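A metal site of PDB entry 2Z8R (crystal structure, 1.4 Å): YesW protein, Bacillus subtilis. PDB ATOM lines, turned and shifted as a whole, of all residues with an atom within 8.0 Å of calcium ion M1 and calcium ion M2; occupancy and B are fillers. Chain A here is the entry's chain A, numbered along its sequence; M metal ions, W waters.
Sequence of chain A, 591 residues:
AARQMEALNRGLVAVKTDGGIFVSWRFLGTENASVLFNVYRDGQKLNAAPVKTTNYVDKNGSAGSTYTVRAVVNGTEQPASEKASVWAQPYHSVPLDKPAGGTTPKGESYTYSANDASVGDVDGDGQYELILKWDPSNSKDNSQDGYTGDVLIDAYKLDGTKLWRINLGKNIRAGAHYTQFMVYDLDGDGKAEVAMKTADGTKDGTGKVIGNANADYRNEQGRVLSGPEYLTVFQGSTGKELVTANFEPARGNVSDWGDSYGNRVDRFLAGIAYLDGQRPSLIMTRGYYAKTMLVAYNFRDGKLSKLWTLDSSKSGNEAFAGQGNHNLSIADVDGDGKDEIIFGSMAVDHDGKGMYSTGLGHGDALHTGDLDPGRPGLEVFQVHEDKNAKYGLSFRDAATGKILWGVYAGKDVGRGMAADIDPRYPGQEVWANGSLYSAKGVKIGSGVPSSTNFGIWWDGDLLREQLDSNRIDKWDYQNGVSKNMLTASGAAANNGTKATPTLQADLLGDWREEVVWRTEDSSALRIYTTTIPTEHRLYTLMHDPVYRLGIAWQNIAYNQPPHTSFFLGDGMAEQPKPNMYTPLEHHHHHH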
ATOM      1  N   ARG A   3       1.167 -17.959 -31.977  1.00  0.00           N
ATOM      2  CA  ARG A   3       1.025 -17.598 -30.563  1.00  0.00           C
ATOM      3  C   ARG A   3      -0.136 -18.310 -29.893  1.00  0.00           C
ATOM      4  O   ARG A   3      -1.203 -18.453 -30.471  1.00  0.00           O
ATOM      5  CB  ARG A   3       0.776 -16.095 -30.403  1.00  0.00           C
ATOM      6  CG  ARG A   3       1.961 -15.252 -30.603  1.00  0.00           C
ATOM      7  CD  ARG A   3       1.626 -13.807 -30.303  1.00  0.00           C
ATOM      8  NE  ARG A   3       2.822 -13.013 -30.508  1.00  0.00           N
ATOM      9  CZ  ARG A   3       3.149 -11.939 -29.792  1.00  0.00           C
ATOM     10  NH1 ARG A   3       2.361 -11.508 -28.804  1.00  0.00           N
ATOM     11  NH2 ARG A   3       4.287 -11.319 -30.078  1.00  0.00           N
ATOM     12  N   TYR A 274       4.643 -11.749 -24.773  1.00  0.00           N
ATOM     13  CA  TYR A 274       5.145 -13.009 -25.365  1.00  0.00           C
ATOM     14  C   TYR A 274       6.638 -12.868 -25.682  1.00  0.00           C
ATOM     15  O   TYR A 274       7.042 -12.666 -26.841  1.00  0.00           O
ATOM     16  CB  TYR A 274       4.326 -13.408 -26.605  1.00  0.00           C
ATOM     17  CG  TYR A 274       2.954 -13.920 -26.279  1.00  0.00           C
ATOM     18  CD1 TYR A 274       2.519 -15.165 -26.756  1.00  0.00           C
ATOM     19  CD2 TYR A 274       2.067 -13.184 -25.483  1.00  0.00           C
ATOM     20  CE1 TYR A 274       1.238 -15.638 -26.459  1.00  0.00           C
ATOM     21  CE2 TYR A 274       0.796 -13.655 -25.176  1.00  0.00           C
ATOM     22  CZ  TYR A 274       0.390 -14.890 -25.665  1.00  0.00           C
ATOM     23  OH  TYR A 274      -0.871 -15.364 -25.377  1.00  0.00           O
ATOM     24  N   LEU A 275       7.455 -12.923 -24.629  1.00  0.00           N
ATOM     25  CA  LEU A 275       8.901 -12.701 -24.754  1.00  0.00           C
ATOM     26  C   LEU A 275       9.601 -13.751 -25.613  1.00  0.00           C
ATOM     27  O   LEU A 275      10.616 -13.454 -26.242  1.00  0.00           O
ATOM     28  CB  LEU A 275       9.556 -12.626 -23.375  1.00  0.00           C
ATOM     29  CG  LEU A 275       8.957 -11.564 -22.446  1.00  0.00           C
ATOM     30  CD1 LEU A 275       9.540 -11.744 -21.047  1.00  0.00           C
ATOM     31  CD2 LEU A 275       9.206 -10.136 -22.954  1.00  0.00           C
ATOM     32  N   GLY A 277       7.944 -15.309 -28.087  1.00  0.00           N
ATOM     33  CA  GLY A 277       7.247 -15.302 -29.381  1.00  0.00           C
ATOM     34  C   GLY A 277       6.127 -16.315 -29.553  1.00  0.00           C
ATOM     35  O   GLY A 277       5.475 -16.346 -30.607  1.00  0.00           O
ATOM     36  N   ALA A 331       4.182  -4.872 -27.514  1.00  0.00           N
ATOM     37  CA  ALA A 331       3.996  -5.193 -28.926  1.00  0.00           C
ATOM     38  C   ALA A 331       5.280  -5.723 -29.525  1.00  0.00           C
ATOM     39  O   ALA A 331       6.354  -5.398 -29.051  1.00  0.00           O
ATOM     40  CB  ALA A 331       3.530  -3.964 -29.700  1.00  0.00           C
ATOM     41  N   ASP A 332       5.149  -6.512 -30.571  1.00  0.00           N
ATOM     42  CA  ASP A 332       6.298  -6.892 -31.388  1.00  0.00           C
ATOM     43  C   ASP A 332       6.593  -5.722 -32.314  1.00  0.00           C
ATOM     44  O   ASP A 332       5.899  -5.507 -33.314  1.00  0.00           O
ATOM     45  CB  ASP A 332       5.999  -8.164 -32.169  1.00  0.00           C
ATOM     46  CG  ASP A 332       7.120  -8.545 -33.111  1.00  0.00           C
ATOM     47  OD1 ASP A 332       8.235  -7.980 -33.015  1.00  0.00           O
ATOM     48  OD2 ASP A 332       6.893  -9.428 -33.954  1.00  0.00           O
ATOM     49  N   VAL A 333       7.597  -4.928 -31.941  1.00  0.00           N
ATOM     50  CA  VAL A 333       7.907  -3.702 -32.666  1.00  0.00           C
ATOM     51  C   VAL A 333       9.005  -3.910 -33.701  1.00  0.00           C
ATOM     52  O   VAL A 333       9.108  -3.147 -34.655  1.00  0.00           O
ATOM     53  CB  VAL A 333       8.299  -2.534 -31.720  1.00  0.00           C
ATOM     54  CG1 VAL A 333       7.192  -2.253 -30.740  1.00  0.00           C
ATOM     55  CG2 VAL A 333       9.620  -2.829 -30.988  1.00  0.00           C
ATOM     56  N   ASP A 334       9.827  -4.942 -33.514  1.00  0.00           N
ATOM     57  CA  ASP A 334      10.992  -5.137 -34.385  1.00  0.00           C
ATOM     58  C   ASP A 334      10.836  -6.278 -35.397  1.00  0.00           C
ATOM     59  O   ASP A 334      11.713  -6.517 -36.228  1.00  0.00           O
ATOM     60  CB  ASP A 334      12.279  -5.287 -33.555  1.00  0.00           C
ATOM     61  CG  ASP A 334      12.234  -6.457 -32.579  1.00  0.00           C
ATOM     62  OD1 ASP A 334      11.369  -7.355 -32.730  1.00  0.00           O
ATOM     63  OD2 ASP A 334      13.078  -6.494 -31.649  1.00  0.00           O
ATOM     64  N   GLY A 335       9.696  -6.979 -35.336  1.00  0.00           N
ATOM     65  CA  GLY A 335       9.343  -8.007 -36.314  1.00  0.00           C
ATOM     66  C   GLY A 335       9.924  -9.402 -36.102  1.00  0.00           C
ATOM     67  O   GLY A 335       9.792 -10.253 -36.986  1.00  0.00           O
ATOM     68  N   ASP A 336      10.537  -9.646 -34.934  1.00  0.00           N
ATOM     69  CA  ASP A 336      11.116 -10.960 -34.615  1.00  0.00           C
ATOM     70  C   ASP A 336      10.105 -11.972 -34.025  1.00  0.00           C
ATOM     71  O   ASP A 336      10.485 -13.092 -33.647  1.00  0.00           O
ATOM     72  CB  ASP A 336      12.378 -10.821 -33.730  1.00  0.00           C
ATOM     73  CG  ASP A 336      12.083 -10.265 -32.341  1.00  0.00           C
ATOM     74  OD1 ASP A 336      10.890 -10.136 -31.967  1.00  0.00           O
ATOM     75  OD2 ASP A 336      13.057  -9.923 -31.605  1.00  0.00           O
ATOM     76  N   GLY A 337       8.826 -11.579 -33.943  1.00  0.00           N
ATOM     77  CA  GLY A 337       7.762 -12.429 -33.394  1.00  0.00           C
ATOM     78  C   GLY A 337       7.573 -12.292 -31.884  1.00  0.00           C
ATOM     79  O   GLY A 337       6.536 -12.709 -31.327  1.00  0.00           O
ATOM     80  N   LYS A 338       8.576 -11.724 -31.218  1.00  0.00           N
ATOM     81  CA  LYS A 338       8.613 -11.624 -29.762  1.00  0.00           C
ATOM     82  C   LYS A 338       8.169 -10.224 -29.353  1.00  0.00           C
ATOM     83  O   LYS A 338       8.355  -9.263 -30.096  1.00  0.00           O
ATOM     84  CB  LYS A 338      10.022 -11.918 -29.257  1.00  0.00           C
ATOM     85  CG  LYS A 338      10.581 -13.227 -29.797  1.00  0.00           C
ATOM     86  CD  LYS A 338      12.016 -13.444 -29.370  1.00  0.00           C
ATOM     87  CE  LYS A 338      12.488 -14.827 -29.803  1.00  0.00           C
ATOM     88  NZ  LYS A 338      13.860 -15.111 -29.274  1.00  0.00           N
ATOM     89  N   ASP A 339       7.564 -10.113 -28.169  1.00  0.00           N
ATOM     90  CA  ASP A 339       7.098  -8.811 -27.686  1.00  0.00           C
ATOM     91  C   ASP A 339       8.170  -7.996 -27.003  1.00  0.00           C
ATOM     92  O   ASP A 339       8.956  -8.499 -26.191  1.00  0.00           O
ATOM     93  CB  ASP A 339       5.926  -8.991 -26.730  1.00  0.00           C
ATOM     94  CG  ASP A 339       4.661  -9.378 -27.443  1.00  0.00           C
ATOM     95  OD1 ASP A 339       4.448  -8.950 -28.601  1.00  0.00           O
ATOM     96  OD2 ASP A 339       3.856 -10.098 -26.822  1.00  0.00           O
ATOM     97  N   GLU A 340       8.149  -6.704 -27.329  1.00  0.00           N
ATOM     98  CA  GLU A 340       8.938  -5.707 -26.641  1.00  0.00           C
ATOM     99  C   GLU A 340       8.008  -4.875 -25.743  1.00  0.00           C
ATOM    100  O   GLU A 340       6.763  -4.969 -25.853  1.00  0.00           O
ATOM    101  CB  GLU A 340       9.680  -4.820 -27.647  1.00  0.00           C
ATOM    102  CG  GLU A 340      10.860  -5.511 -28.366  1.00  0.00           C
ATOM    103  CD  GLU A 340      10.439  -6.501 -29.452  1.00  0.00           C
ATOM    104  OE1 GLU A 340       9.561  -6.207 -30.290  1.00  0.00           O
ATOM    105  OE2 GLU A 340      11.038  -7.613 -29.498  1.00  0.00           O
ATOM    106  N   ILE A 341       8.607  -4.085 -24.878  1.00  0.00           N
ATOM    107  CA  ILE A 341       7.865  -3.288 -23.899  1.00  0.00           C
ATOM    108  C   ILE A 341       8.101  -1.806 -24.191  1.00  0.00           C
ATOM    109  O   ILE A 341       9.244  -1.350 -24.188  1.00  0.00           O
ATOM    110  CB  ILE A 341       8.312  -3.617 -22.464  1.00  0.00           C
ATOM    111  CG1 ILE A 341       8.069  -5.101 -22.164  1.00  0.00           C
ATOM    112  CG2 ILE A 341       7.579  -2.743 -21.438  1.00  0.00           C
ATOM    113  CD1 ILE A 341       8.964  -5.660 -21.058  1.00  0.00           C
ATOM    114  N   VAL A 348      12.093  -1.580 -23.963  1.00  0.00           N
ATOM    115  CA  VAL A 348      12.862  -2.706 -23.434  1.00  0.00           C
ATOM    116  C   VAL A 348      12.618  -3.892 -24.346  1.00  0.00           C
ATOM    117  O   VAL A 348      11.471  -4.175 -24.692  1.00  0.00           O
ATOM    118  CB  VAL A 348      12.444  -3.056 -21.983  1.00  0.00           C
ATOM    119  CG1 VAL A 348      13.276  -4.243 -21.444  1.00  0.00           C
ATOM    120  CG2 VAL A 348      12.612  -1.843 -21.077  1.00  0.00           C
ATOM    121  N   ASP A 349      13.702  -4.557 -24.739  1.00  0.00           N
ATOM    122  CA  ASP A 349      13.624  -5.688 -25.648  1.00  0.00           C
ATOM    123  C   ASP A 349      13.090  -6.943 -24.958  1.00  0.00           C
ATOM    124  O   ASP A 349      13.004  -7.002 -23.738  1.00  0.00           O
ATOM    125  CB  ASP A 349      15.022  -5.979 -26.220  1.00  0.00           C
ATOM    126  CG  ASP A 349      14.991  -6.516 -27.654  1.00  0.00           C
ATOM    127  OD1 ASP A 349      13.895  -6.878 -28.174  1.00  0.00           O
ATOM    128  OD2 ASP A 349      16.089  -6.571 -28.262  1.00  0.00           O
ATOM    129  N   HIS A 350      12.755  -7.944 -25.771  1.00  0.00           N
ATOM    130  CA  HIS A 350      12.156  -9.183 -25.276  1.00  0.00           C
ATOM    131  C   HIS A 350      13.067  -9.944 -24.303  1.00  0.00           C
ATOM    132  O   HIS A 350      12.611 -10.824 -23.576  1.00  0.00           O
ATOM    133  CB  HIS A 350      11.783 -10.082 -26.457  1.00  0.00           C
ATOM    134  CG  HIS A 350      12.978 -10.641 -27.162  1.00  0.00           C
ATOM    135  ND1 HIS A 350      13.525 -10.064 -28.294  1.00  0.00           N
ATOM    136  CD2 HIS A 350      13.763 -11.693 -26.862  1.00  0.00           C
ATOM    137  CE1 HIS A 350      14.581 -10.768 -28.669  1.00  0.00           C
ATOM    138  NE2 HIS A 350      14.751 -11.760 -27.815  1.00  0.00           N
ATOM    139  N   ASP A 351      14.362  -9.617 -24.325  1.00  0.00           N
ATOM    140  CA  ASP A 351      15.357 -10.275 -23.466  1.00  0.00           C
ATOM    141  C   ASP A 351      15.755  -9.404 -22.271  1.00  0.00           C
ATOM    142  O   ASP A 351      16.690  -9.716 -21.554  1.00  0.00           O
ATOM    143  CB  ASP A 351      16.616 -10.625 -24.269  1.00  0.00           C
ATOM    144  CG  ASP A 351      17.248  -9.419 -24.926  1.00  0.00           C
ATOM    145  OD1 ASP A 351      16.771  -8.282 -24.744  1.00  0.00           O
ATOM    146  OD2 ASP A 351      18.257  -9.600 -25.642  1.00  0.00           O
ATOM    147  N   MET A 355      16.433  -0.805 -25.101  1.00  0.00           N
ATOM    148  CA  MET A 355      16.533  -0.576 -26.550  1.00  0.00           C
ATOM    149  C   MET A 355      16.893   0.851 -26.913  1.00  0.00           C
ATOM    150  O   MET A 355      17.795   1.097 -27.720  1.00  0.00           O
ATOM    151  CB  MET A 355      15.205  -0.939 -27.229  1.00  0.00           C
ATOM    152  CG  MET A 355      14.939  -2.421 -27.302  1.00  0.00           C
ATOM    153  SD  MET A 355      13.198  -2.784 -27.553  1.00  0.00           S
ATOM    154  CE  MET A 355      12.851  -1.980 -29.123  1.00  0.00           C
HETATM  155 CA    CA M   1      13.214  -8.219 -30.006  1.00  0.00          CA
HETATM  156 CA    CA M   2       9.864  -8.268 -31.433  1.00  0.00          CA
HETATM  157  O   HOH W   1      15.590  -8.147 -30.378  1.00  0.00           O
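The side-chain carboxylate (OD1) of Asp 332 sits close to the backbone NH (N) of Gly 335, at 2.9 Å. OD2 of Asp 332 sits at hydrogen-bond distance from N of Gly 337, at 2.9 Å. The side-chain carboxylate (OD1) of Asp 339 is in hydrogen-bond range of the backbone NH (N) of Asp 332. OE1 of Glu 340 lies close to N of Val 333, 2.9 Å away. O of Ala 331 lies within hydrogen-bond range of N of Glu 340 (2.8 Å). N of Asp 349 sits at hydrogen-bond distance from SD of Met 355 (3.4 Å).
Of the 20 residues printed, 5 come within 4 Å of calcium ion M1. The nearest printed residue that does not touch calcium ion M1 is Lys 338 (4.9 Å).
Five residues have an atom within 4 Å of calcium ion M2: Asp 332, Asp 334, Asp 336, Lys 338 and Glu 340. The nearest printed residue that does not touch calcium ion M2 is Val 333 (4.1 Å).
Calcium ion M1 is bound by OE2 of Glu 340, OD2 of Asp 336, OD1 of Asp 349, OD2 of Asp 334, water W1 and ND1 of His 350. Calcium ion M1 has six donor atoms within binding distance.
Calcium ion M2 is bound by the side-chain carboxylate (OD1) of Asp 334 (2.2 Å), the side-chain carboxylate (OD1) of Asp 336 (2.2 Å), the backbone carbonyl oxygen (O) of Lys 338 (2.2 Å), the side-chain carboxylate (OD1) of Asp 332 (2.3 Å), the side-chain carboxylate (OE2) of Glu 340 (2.4 Å) and the side-chain carboxylate (OE1) of Glu 340 (2.4 Å). Calcium ion M2 has six donor atoms within binding distance.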
